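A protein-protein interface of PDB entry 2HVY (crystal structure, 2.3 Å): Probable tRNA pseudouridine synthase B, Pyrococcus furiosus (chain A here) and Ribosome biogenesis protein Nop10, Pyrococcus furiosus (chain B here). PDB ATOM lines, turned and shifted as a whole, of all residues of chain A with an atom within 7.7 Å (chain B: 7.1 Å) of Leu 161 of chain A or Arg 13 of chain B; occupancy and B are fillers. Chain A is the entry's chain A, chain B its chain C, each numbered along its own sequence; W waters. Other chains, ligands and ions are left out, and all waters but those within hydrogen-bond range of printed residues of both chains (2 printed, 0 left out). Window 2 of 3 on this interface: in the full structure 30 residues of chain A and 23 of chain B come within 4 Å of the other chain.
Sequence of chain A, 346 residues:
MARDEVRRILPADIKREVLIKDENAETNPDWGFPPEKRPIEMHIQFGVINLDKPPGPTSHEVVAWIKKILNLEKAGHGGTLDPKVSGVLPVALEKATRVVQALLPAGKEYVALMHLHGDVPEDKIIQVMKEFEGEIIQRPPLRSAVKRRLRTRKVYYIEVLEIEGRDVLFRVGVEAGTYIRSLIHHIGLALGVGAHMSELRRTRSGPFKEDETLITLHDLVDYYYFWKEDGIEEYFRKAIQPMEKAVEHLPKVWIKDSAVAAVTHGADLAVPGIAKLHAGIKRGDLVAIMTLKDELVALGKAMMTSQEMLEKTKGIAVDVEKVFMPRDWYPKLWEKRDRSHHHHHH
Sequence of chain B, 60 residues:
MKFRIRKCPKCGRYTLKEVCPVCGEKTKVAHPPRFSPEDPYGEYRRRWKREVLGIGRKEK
Water W1 lies within hydrogen-bond range of the backbone carbonyl oxygen of Tyr 14 of chain B, the side-chain carboxylate of Glu 162 of chain A and the guanidinium group of Arg 13 of chain B.
Water W2 bridges NH2 of Arg 171 of chain A and N of Tyr 14 of chain B.
Of the printed residues of chain B, Val 111 of chain A touches Tyr 14 (3.6 Å).
Of the printed residues of chain B, Leu 161 of chain A touches Arg 13 (3.0 Å) and Tyr 14 (3.8 Å).
Of the printed residues of chain B, Glu 162 of chain A touches Thr 15 and Leu 16.
Of the printed residues of chain B, Leu 169 of chain A touches Tyr 14 (3.7 Å) and Thr 15 (3.6 Å).
Pro 9 of chain B touches none of the printed residues of chain A.
No residue of chain A comes within 4 Å of Gly 12 of chain B.
Arg 13 of chain B touches just one residue of chain A: Leu 161 (3.0 Å).
Of the printed residues of chain A, Thr 15 of chain B touches Glu 162 and Leu 169.
Printed residues of chain A within 4 Å of Leu 16 of chain B: Glu 162 (2.7 Å).
Thr 27 of chain B touches none of the printed residues of chain A.
Hydrophobic or aromatic side chains of chain A within 4 Å of the printed part of chain B: Val 111, Leu 161 and Leu 169.
Of the 17 printed residues of chain B, 4 touch a printed residue of chain A.
Printed residues of chain B that touch a printed residue of chain A: Arg 13, Tyr 14, Thr 15 and Leu 16.
Among the printed residues, 8 pairs touch across the chains.
Among the printed residues, no Asp or Glu carboxylate lies within 4 Å of a Lys or Arg side-chain nitrogen of the other chain.
NH2 of Arg 13 of chain B is in hydrogen-bond range of O of Leu 161 of chain A.
The side-chain carboxylate (OE2) of Glu 162 of chain A lies within hydrogen-bond range of the side-chain hydroxyl (OG1) of Thr 15 of chain B (2.7 Å).
The side-chain carboxylate (OE1) of Glu 162 of chain A lies within hydrogen-bond range of the backbone NH (N) of Leu 16 of chain B, 2.7 Å away.
Among the printed residues, pairs that only touch across the chains: Arg 171 of chain A with Tyr 14 of chain B (3.4 Å), Leu 169 of chain A with Thr 15 of chain B (3.6 Å), Val 111 of chain A with Tyr 14 of chain B (3.6 Å), Leu 169 of chain A with Tyr 14 of chain B (3.7 Å) and Leu 161 of chain A with Tyr 14 of chain B (3.8 Å).
The backbone carbonyl oxygen (O) of Arg 171 of chain A lies within hydrogen-bond range of the backbone NH (N) of Glu 159 of chain A, at 2.8 Å.
O of Leu 169 of chain A sits at hydrogen-bond distance from N of Leu 161 of chain A, at 2.8 Å.
N of Leu 169 of chain A sits at hydrogen-bond distance from O of Glu 162 of chain A.
N of Arg 6 of chain B sits at hydrogen-bond distance from O of Thr 15 of chain B (2.8 Å).
The backbone NH of Cys 8 of chain B sits at hydrogen-bond distance from the backbone carbonyl oxygen of Arg 13 of chain B (2.9 Å).
SG of Cys 11 of chain B sits close to N of Arg 13 of chain B, 3.7 Å away.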
ATOM      1  N   TYR A 110       9.979 -25.820  20.287  1.00  0.00           N
ATOM      2  CA  TYR A 110      10.043 -25.300  21.647  1.00  0.00           C
ATOM      3  C   TYR A 110       8.764 -25.602  22.411  1.00  0.00           C
ATOM      4  O   TYR A 110       7.695 -25.762  21.819  1.00  0.00           O
ATOM      5  CB  TYR A 110      10.236 -23.781  21.641  1.00  0.00           C
ATOM      6  CG  TYR A 110      11.510 -23.267  21.011  1.00  0.00           C
ATOM      7  CD1 TYR A 110      11.564 -22.966  19.651  1.00  0.00           C
ATOM      8  CD2 TYR A 110      12.650 -23.042  21.780  1.00  0.00           C
ATOM      9  CE1 TYR A 110      12.726 -22.477  19.069  1.00  0.00           C
ATOM     10  CE2 TYR A 110      13.818 -22.550  21.209  1.00  0.00           C
ATOM     11  CZ  TYR A 110      13.848 -22.270  19.852  1.00  0.00           C
ATOM     12  OH  TYR A 110      15.001 -21.782  19.279  1.00  0.00           O
ATOM     13  N   VAL A 111       8.892 -25.685  23.731  1.00  0.00           N
ATOM     14  CA  VAL A 111       7.761 -25.563  24.636  1.00  0.00           C
ATOM     15  C   VAL A 111       7.961 -24.242  25.375  1.00  0.00           C
ATOM     16  O   VAL A 111       9.018 -24.008  25.966  1.00  0.00           O
ATOM     17  CB  VAL A 111       7.661 -26.758  25.617  1.00  0.00           C
ATOM     18  CG1 VAL A 111       6.591 -26.514  26.678  1.00  0.00           C
ATOM     19  CG2 VAL A 111       7.358 -28.040  24.856  1.00  0.00           C
ATOM     20  N   ALA A 112       6.951 -23.381  25.314  1.00  0.00           N
ATOM     21  CA  ALA A 112       7.041 -22.036  25.868  1.00  0.00           C
ATOM     22  C   ALA A 112       5.880 -21.737  26.804  1.00  0.00           C
ATOM     23  O   ALA A 112       4.775 -22.263  26.630  1.00  0.00           O
ATOM     24  CB  ALA A 112       7.087 -21.008  24.743  1.00  0.00           C
ATOM     25  N   MET A 129      -3.816 -17.512  18.323  1.00  0.00           N
ATOM     26  CA  MET A 129      -2.585 -18.294  18.197  1.00  0.00           C
ATOM     27  C   MET A 129      -2.581 -19.180  16.950  1.00  0.00           C
ATOM     28  O   MET A 129      -1.527 -19.411  16.358  1.00  0.00           O
ATOM     29  CB  MET A 129      -2.320 -19.114  19.465  1.00  0.00           C
ATOM     30  CG  MET A 129      -1.942 -18.254  20.664  1.00  0.00           C
ATOM     31  SD  MET A 129      -1.547 -19.182  22.155  1.00  0.00           S
ATOM     32  CE  MET A 129       0.178 -19.561  21.864  1.00  0.00           C
ATOM     33  N   ILE A 158       1.425 -24.465  16.036  1.00  0.00           N
ATOM     34  CA  ILE A 158       1.292 -24.072  17.432  1.00  0.00           C
ATOM     35  C   ILE A 158       0.254 -24.990  18.077  1.00  0.00           C
ATOM     36  O   ILE A 158      -0.884 -25.081  17.611  1.00  0.00           O
ATOM     37  CB  ILE A 158       0.898 -22.575  17.593  1.00  0.00           C
ATOM     38  CG1 ILE A 158       2.037 -21.667  17.114  1.00  0.00           C
ATOM     39  CG2 ILE A 158       0.544 -22.255  19.052  1.00  0.00           C
ATOM     40  CD1 ILE A 158       1.650 -20.207  16.917  1.00  0.00           C
ATOM     41  N   GLU A 159       0.666 -25.689  19.132  1.00  0.00           N
ATOM     42  CA  GLU A 159      -0.225 -26.575  19.875  1.00  0.00           C
ATOM     43  C   GLU A 159      -0.369 -26.064  21.302  1.00  0.00           C
ATOM     44  O   GLU A 159       0.559 -26.184  22.107  1.00  0.00           O
ATOM     45  CB  GLU A 159       0.312 -28.015  19.869  1.00  0.00           C
ATOM     46  CG  GLU A 159      -0.583 -29.034  20.589  1.00  0.00           C
ATOM     47  CD  GLU A 159       0.115 -30.360  20.885  1.00  0.00           C
ATOM     48  OE1 GLU A 159      -0.552 -31.279  21.409  1.00  0.00           O
ATOM     49  OE2 GLU A 159       1.327 -30.490  20.602  1.00  0.00           O
ATOM     50  N   VAL A 160      -1.526 -25.481  21.607  1.00  0.00           N
ATOM     51  CA  VAL A 160      -1.831 -25.040  22.966  1.00  0.00           C
ATOM     52  C   VAL A 160      -2.064 -26.267  23.846  1.00  0.00           C
ATOM     53  O   VAL A 160      -2.998 -27.042  23.619  1.00  0.00           O
ATOM     54  CB  VAL A 160      -3.050 -24.083  23.017  1.00  0.00           C
ATOM     55  CG1 VAL A 160      -3.383 -23.706  24.458  1.00  0.00           C
ATOM     56  CG2 VAL A 160      -2.787 -22.828  22.194  1.00  0.00           C
ATOM     57  N   LEU A 161      -1.198 -26.441  24.840  1.00  0.00           N
ATOM     58  CA  LEU A 161      -1.256 -27.602  25.724  1.00  0.00           C
ATOM     59  C   LEU A 161      -2.243 -27.393  26.870  1.00  0.00           C
ATOM     60  O   LEU A 161      -3.096 -28.247  27.121  1.00  0.00           O
ATOM     61  CB  LEU A 161       0.141 -27.961  26.245  1.00  0.00           C
ATOM     62  CG  LEU A 161       1.185 -28.306  25.173  1.00  0.00           C
ATOM     63  CD1 LEU A 161       2.592 -28.334  25.756  1.00  0.00           C
ATOM     64  CD2 LEU A 161       0.859 -29.625  24.471  1.00  0.00           C
ATOM     65  N   GLU A 162      -2.127 -26.257  27.555  1.00  0.00           N
ATOM     66  CA  GLU A 162      -3.068 -25.888  28.616  1.00  0.00           C
ATOM     67  C   GLU A 162      -3.057 -24.393  28.934  1.00  0.00           C
ATOM     68  O   GLU A 162      -2.046 -23.712  28.759  1.00  0.00           O
ATOM     69  CB  GLU A 162      -2.834 -26.717  29.894  1.00  0.00           C
ATOM     70  CG  GLU A 162      -1.411 -26.702  30.441  1.00  0.00           C
ATOM     71  CD  GLU A 162      -1.238 -27.639  31.629  1.00  0.00           C
ATOM     72  OE1 GLU A 162      -0.906 -27.146  32.726  1.00  0.00           O
ATOM     73  OE2 GLU A 162      -1.445 -28.864  31.473  1.00  0.00           O
ATOM     74  N   ILE A 163      -4.203 -23.897  29.392  1.00  0.00           N
ATOM     75  CA  ILE A 163      -4.338 -22.514  29.836  1.00  0.00           C
ATOM     76  C   ILE A 163      -4.707 -22.504  31.319  1.00  0.00           C
ATOM     77  O   ILE A 163      -5.726 -23.069  31.720  1.00  0.00           O
ATOM     78  CB  ILE A 163      -5.379 -21.728  28.988  1.00  0.00           C
ATOM     79  CG1 ILE A 163      -4.898 -21.597  27.540  1.00  0.00           C
ATOM     80  CG2 ILE A 163      -5.643 -20.343  29.592  1.00  0.00           C
ATOM     81  CD1 ILE A 163      -6.003 -21.370  26.521  1.00  0.00           C
ATOM     82  N   VAL A 168      -0.304 -19.441  29.451  1.00  0.00           N
ATOM     83  CA  VAL A 168      -0.583 -20.288  28.296  1.00  0.00           C
ATOM     84  C   VAL A 168       0.657 -21.111  27.943  1.00  0.00           C
ATOM     85  O   VAL A 168       1.682 -20.567  27.523  1.00  0.00           O
ATOM     86  CB  VAL A 168      -1.068 -19.473  27.064  1.00  0.00           C
ATOM     87  CG1 VAL A 168      -1.312 -20.390  25.865  1.00  0.00           C
ATOM     88  CG2 VAL A 168      -2.338 -18.691  27.393  1.00  0.00           C
ATOM     89  N   LEU A 169       0.549 -22.422  28.135  1.00  0.00           N
ATOM     90  CA  LEU A 169       1.617 -23.353  27.796  1.00  0.00           C
ATOM     91  C   LEU A 169       1.371 -23.928  26.408  1.00  0.00           C
ATOM     92  O   LEU A 169       0.305 -24.481  26.136  1.00  0.00           O
ATOM     93  CB  LEU A 169       1.702 -24.475  28.835  1.00  0.00           C
ATOM     94  CG  LEU A 169       2.849 -25.482  28.704  1.00  0.00           C
ATOM     95  CD1 LEU A 169       4.182 -24.861  29.109  1.00  0.00           C
ATOM     96  CD2 LEU A 169       2.556 -26.706  29.544  1.00  0.00           C
ATOM     97  N   PHE A 170       2.360 -23.793  25.532  1.00  0.00           N
ATOM     98  CA  PHE A 170       2.216 -24.252  24.156  1.00  0.00           C
ATOM     99  C   PHE A 170       3.502 -24.793  23.545  1.00  0.00           C
ATOM    100  O   PHE A 170       4.606 -24.383  23.911  1.00  0.00           O
ATOM    101  CB  PHE A 170       1.606 -23.151  23.271  1.00  0.00           C
ATOM    102  CG  PHE A 170       2.520 -21.978  23.019  1.00  0.00           C
ATOM    103  CD1 PHE A 170       3.163 -21.838  21.793  1.00  0.00           C
ATOM    104  CD2 PHE A 170       2.709 -20.996  23.993  1.00  0.00           C
ATOM    105  CE1 PHE A 170       4.002 -20.748  21.543  1.00  0.00           C
ATOM    106  CE2 PHE A 170       3.541 -19.903  23.756  1.00  0.00           C
ATOM    107  CZ  PHE A 170       4.188 -19.777  22.528  1.00  0.00           C
ATOM    108  N   ARG A 171       3.335 -25.730  22.617  1.00  0.00           N
ATOM    109  CA  ARG A 171       4.434 -26.243  21.817  1.00  0.00           C
ATOM    110  C   ARG A 171       4.420 -25.542  20.459  1.00  0.00           C
ATOM    111  O   ARG A 171       3.354 -25.284  19.899  1.00  0.00           O
ATOM    112  CB  ARG A 171       4.306 -27.758  21.649  1.00  0.00           C
ATOM    113  CG  ARG A 171       5.613 -28.459  21.331  1.00  0.00           C
ATOM    114  CD  ARG A 171       5.394 -29.928  21.002  1.00  0.00           C
ATOM    115  NE  ARG A 171       5.225 -30.762  22.193  1.00  0.00           N
ATOM    116  CZ  ARG A 171       6.178 -31.528  22.725  1.00  0.00           C
ATOM    117  NH1 ARG A 171       7.393 -31.576  22.186  1.00  0.00           N
ATOM    118  NH2 ARG A 171       5.913 -32.254  23.806  1.00  0.00           N
ATOM    119  N   VAL A 172       5.603 -25.229  19.939  1.00  0.00           N
ATOM    120  CA  VAL A 172       5.715 -24.479  18.693  1.00  0.00           C
ATOM    121  C   VAL A 172       6.895 -24.958  17.839  1.00  0.00           C
ATOM    122  O   VAL A 172       8.021 -25.069  18.318  1.00  0.00           O
ATOM    123  CB  VAL A 172       5.746 -22.928  18.945  1.00  0.00           C
ATOM    124  CG1 VAL A 172       6.923 -22.514  19.843  1.00  0.00           C
ATOM    125  CG2 VAL A 172       5.745 -22.147  17.633  1.00  0.00           C
ATOM    126  N   ARG B   6       6.502 -28.217  33.691  1.00  0.00           N
ATOM    127  CA  ARG B   6       6.743 -29.573  34.173  1.00  0.00           C
ATOM    128  C   ARG B   6       6.529 -30.583  33.051  1.00  0.00           C
ATOM    129  O   ARG B   6       5.977 -30.252  32.000  1.00  0.00           O
ATOM    130  CB  ARG B   6       5.847 -29.900  35.378  1.00  0.00           C
ATOM    131  CG  ARG B   6       5.882 -28.875  36.510  1.00  0.00           C
ATOM    132  CD  ARG B   6       5.425 -29.485  37.829  1.00  0.00           C
ATOM    133  NE  ARG B   6       6.560 -29.987  38.602  1.00  0.00           N
ATOM    134  CZ  ARG B   6       6.488 -30.926  39.540  1.00  0.00           C
ATOM    135  NH1 ARG B   6       5.328 -31.498  39.837  1.00  0.00           N
ATOM    136  NH2 ARG B   6       7.586 -31.303  40.179  1.00  0.00           N
ATOM    137  N   LYS B   7       6.978 -31.813  33.276  1.00  0.00           N
ATOM    138  CA  LYS B   7       6.842 -32.878  32.293  1.00  0.00           C
ATOM    139  C   LYS B   7       6.546 -34.210  32.974  1.00  0.00           C
ATOM    140  O   LYS B   7       7.136 -34.532  34.005  1.00  0.00           O
ATOM    141  CB  LYS B   7       8.114 -32.986  31.439  1.00  0.00           C
ATOM    142  CG  LYS B   7       7.978 -33.879  30.217  1.00  0.00           C
ATOM    143  CD  LYS B   7       9.294 -34.004  29.463  1.00  0.00           C
ATOM    144  CE  LYS B   7       9.083 -34.707  28.135  1.00  0.00           C
ATOM    145  NZ  LYS B   7      10.328 -34.784  27.327  1.00  0.00           N
ATOM    146  N   CYS B   8       5.620 -34.971  32.393  1.00  0.00           N
ATOM    147  CA  CYS B   8       5.373 -36.341  32.823  1.00  0.00           C
ATOM    148  C   CYS B   8       6.516 -37.234  32.343  1.00  0.00           C
ATOM    149  O   CYS B   8       6.825 -37.254  31.150  1.00  0.00           O
ATOM    150  CB  CYS B   8       4.038 -36.848  32.282  1.00  0.00           C
ATOM    151  SG  CYS B   8       3.594 -38.510  32.852  1.00  0.00           S
ATOM    152  N   PRO B   9       7.155 -37.969  33.273  1.00  0.00           N
ATOM    153  CA  PRO B   9       8.323 -38.791  32.941  1.00  0.00           C
ATOM    154  C   PRO B   9       8.004 -39.980  32.035  1.00  0.00           C
ATOM    155  O   PRO B   9       8.848 -40.380  31.231  1.00  0.00           O
ATOM    156  CB  PRO B   9       8.808 -39.292  34.312  1.00  0.00           C
ATOM    157  CG  PRO B   9       8.119 -38.434  35.322  1.00  0.00           C
ATOM    158  CD  PRO B   9       6.816 -38.064  34.704  1.00  0.00           C
ATOM    159  N   LYS B  10       6.797 -40.527  32.159  1.00  0.00           N
ATOM    160  CA  LYS B  10       6.430 -41.760  31.459  1.00  0.00           C
ATOM    161  C   LYS B  10       5.783 -41.560  30.085  1.00  0.00           C
ATOM    162  O   LYS B  10       6.064 -42.319  29.155  1.00  0.00           O
ATOM    163  CB  LYS B  10       5.553 -42.653  32.349  1.00  0.00           C
ATOM    164  CG  LYS B  10       6.329 -43.667  33.195  1.00  0.00           C
ATOM    165  CD  LYS B  10       7.139 -43.006  34.309  1.00  0.00           C
ATOM    166  CE  LYS B  10       8.089 -43.992  34.966  1.00  0.00           C
ATOM    167  NZ  LYS B  10       8.963 -43.324  35.972  1.00  0.00           N
ATOM    168  N   CYS B  11       4.921 -40.552  29.957  1.00  0.00           N
ATOM    169  CA  CYS B  11       4.231 -40.304  28.687  1.00  0.00           C
ATOM    170  C   CYS B  11       4.759 -39.080  27.926  1.00  0.00           C
ATOM    171  O   CYS B  11       4.426 -38.878  26.757  1.00  0.00           O
ATOM    172  CB  CYS B  11       2.710 -40.235  28.881  1.00  0.00           C
ATOM    173  SG  CYS B  11       2.061 -38.626  29.368  1.00  0.00           S
ATOM    174  N   GLY B  12       5.572 -38.270  28.600  1.00  0.00           N
ATOM    175  CA  GLY B  12       6.250 -37.136  27.967  1.00  0.00           C
ATOM    176  C   GLY B  12       5.401 -35.899  27.741  1.00  0.00           C
ATOM    177  O   GLY B  12       5.743 -35.053  26.915  1.00  0.00           O
ATOM    178  N   ARG B  13       4.298 -35.792  28.480  1.00  0.00           N
ATOM    179  CA  ARG B  13       3.380 -34.659  28.362  1.00  0.00           C
ATOM    180  C   ARG B  13       3.902 -33.440  29.122  1.00  0.00           C
ATOM    181  O   ARG B  13       4.245 -33.532  30.304  1.00  0.00           O
ATOM    182  CB  ARG B  13       1.986 -35.055  28.874  1.00  0.00           C
ATOM    183  CG  ARG B  13       0.962 -33.921  28.975  1.00  0.00           C
ATOM    184  CD  ARG B  13       0.281 -33.652  27.647  1.00  0.00           C
ATOM    185  NE  ARG B  13      -0.678 -32.551  27.731  1.00  0.00           N
ATOM    186  CZ  ARG B  13      -1.501 -32.191  26.748  1.00  0.00           C
ATOM    187  NH1 ARG B  13      -1.498 -32.845  25.593  1.00  0.00           N
ATOM    188  NH2 ARG B  13      -2.333 -31.174  26.921  1.00  0.00           N
ATOM    189  N   TYR B  14       3.964 -32.303  28.436  1.00  0.00           N
ATOM    190  CA  TYR B  14       4.291 -31.041  29.085  1.00  0.00           C
ATOM    191  C   TYR B  14       3.054 -30.425  29.730  1.00  0.00           C
ATOM    192  O   TYR B  14       1.983 -30.382  29.122  1.00  0.00           O
ATOM    193  CB  TYR B  14       4.948 -30.072  28.102  1.00  0.00           C
ATOM    194  CG  TYR B  14       6.427 -30.324  27.930  1.00  0.00           C
ATOM    195  CD1 TYR B  14       6.913 -31.035  26.832  1.00  0.00           C
ATOM    196  CD2 TYR B  14       7.339 -29.871  28.880  1.00  0.00           C
ATOM    197  CE1 TYR B  14       8.277 -31.272  26.680  1.00  0.00           C
ATOM    198  CE2 TYR B  14       8.697 -30.104  28.740  1.00  0.00           C
ATOM    199  CZ  TYR B  14       9.160 -30.802  27.643  1.00  0.00           C
ATOM    200  OH  TYR B  14      10.507 -31.021  27.522  1.00  0.00           O
ATOM    201  N   THR B  15       3.216 -29.970  30.971  1.00  0.00           N
ATOM    202  CA  THR B  15       2.110 -29.445  31.772  1.00  0.00           C
ATOM    203  C   THR B  15       2.608 -28.460  32.834  1.00  0.00           C
ATOM    204  O   THR B  15       3.811 -28.355  33.076  1.00  0.00           O
ATOM    205  CB  THR B  15       1.286 -30.590  32.439  1.00  0.00           C
ATOM    206  OG1 THR B  15       0.212 -30.036  33.204  1.00  0.00           O
ATOM    207  CG2 THR B  15       2.155 -31.444  33.353  1.00  0.00           C
ATOM    208  N   LEU B  16       1.673 -27.735  33.444  1.00  0.00           N
ATOM    209  CA  LEU B  16       1.967 -26.893  34.603  1.00  0.00           C
ATOM    210  C   LEU B  16       1.479 -27.564  35.887  1.00  0.00           C
ATOM    211  O   LEU B  16       1.769 -27.098  36.991  1.00  0.00           O
ATOM    212  CB  LEU B  16       1.320 -25.509  34.453  1.00  0.00           C
ATOM    213  CG  LEU B  16       1.634 -24.678  33.202  1.00  0.00           C
ATOM    214  CD1 LEU B  16       0.729 -23.454  33.135  1.00  0.00           C
ATOM    215  CD2 LEU B  16       3.105 -24.272  33.144  1.00  0.00           C
ATOM    216  N   CYS B  20      -0.233 -35.544  35.924  1.00  0.00           N
ATOM    217  CA  CYS B  20      -0.357 -35.574  34.472  1.00  0.00           C
ATOM    218  C   CYS B  20      -1.828 -35.646  34.052  1.00  0.00           C
ATOM    219  O   CYS B  20      -2.571 -36.496  34.543  1.00  0.00           O
ATOM    220  CB  CYS B  20       0.431 -36.746  33.889  1.00  0.00           C
ATOM    221  SG  CYS B  20       0.434 -36.803  32.084  1.00  0.00           S
ATOM    222  N   PRO B  21      -2.253 -34.744  33.143  1.00  0.00           N
ATOM    223  CA  PRO B  21      -3.644 -34.707  32.688  1.00  0.00           C
ATOM    224  C   PRO B  21      -4.025 -35.884  31.783  1.00  0.00           C
ATOM    225  O   PRO B  21      -5.213 -36.109  31.538  1.00  0.00           O
ATOM    226  CB  PRO B  21      -3.721 -33.389  31.912  1.00  0.00           C
ATOM    227  CG  PRO B  21      -2.336 -33.158  31.430  1.00  0.00           C
ATOM    228  CD  PRO B  21      -1.437 -33.694  32.502  1.00  0.00           C
ATOM    229  N   VAL B  22      -3.025 -36.622  31.303  1.00  0.00           N
ATOM    230  CA  VAL B  22      -3.250 -37.737  30.381  1.00  0.00           C
ATOM    231  C   VAL B  22      -3.341 -39.084  31.107  1.00  0.00           C
ATOM    232  O   VAL B  22      -4.360 -39.772  31.012  1.00  0.00           O
ATOM    233  CB  VAL B  22      -2.171 -37.784  29.258  1.00  0.00           C
ATOM    234  CG1 VAL B  22      -2.396 -38.974  28.332  1.00  0.00           C
ATOM    235  CG2 VAL B  22      -2.175 -36.488  28.458  1.00  0.00           C
ATOM    236  N   CYS B  23      -2.284 -39.449  31.832  1.00  0.00           N
ATOM    237  CA  CYS B  23      -2.209 -40.759  32.489  1.00  0.00           C
ATOM    238  C   CYS B  23      -2.424 -40.708  34.003  1.00  0.00           C
ATOM    239  O   CYS B  23      -2.776 -41.720  34.615  1.00  0.00           O
ATOM    240  CB  CYS B  23      -0.886 -41.455  32.157  1.00  0.00           C
ATOM    241  SG  CYS B  23       0.582 -40.587  32.731  1.00  0.00           S
ATOM    242  N   THR B  27       4.349 -35.334  38.007  1.00  0.00           N
ATOM    243  CA  THR B  27       5.210 -34.740  36.990  1.00  0.00           C
ATOM    244  C   THR B  27       6.518 -34.243  37.594  1.00  0.00           C
ATOM    245  O   THR B  27       6.614 -34.027  38.805  1.00  0.00           O
ATOM    246  CB  THR B  27       4.509 -33.572  36.267  1.00  0.00           C
ATOM    247  OG1 THR B  27       4.086 -32.597  37.228  1.00  0.00           O
ATOM    248  CG2 THR B  27       3.304 -34.070  35.479  1.00  0.00           C
ATOM    249  N   LYS B  28       7.522 -34.077  36.740  1.00  0.00           N
ATOM    250  CA  LYS B  28       8.809 -33.532  37.163  1.00  0.00           C
ATOM    251  C   LYS B  28       9.107 -32.227  36.434  1.00  0.00           C
ATOM    252  O   LYS B  28       8.648 -32.021  35.311  1.00  0.00           O
ATOM    253  CB  LYS B  28       9.930 -34.550  36.941  1.00  0.00           C
ATOM    254  CG  LYS B  28       9.949 -35.676  37.963  1.00  0.00           C
ATOM    255  CD  LYS B  28      11.318 -36.328  38.038  1.00  0.00           C
ATOM    256  CE  LYS B  28      11.474 -37.139  39.313  1.00  0.00           C
ATOM    257  NZ  LYS B  28      12.888 -37.548  39.540  1.00  0.00           N
HETATM  258  O   HOH W   1      -0.672 -30.314  29.298  1.00  0.00           O
HETATM  259  O   HOH W   2       3.589 -32.137  25.383  1.00  0.00           O
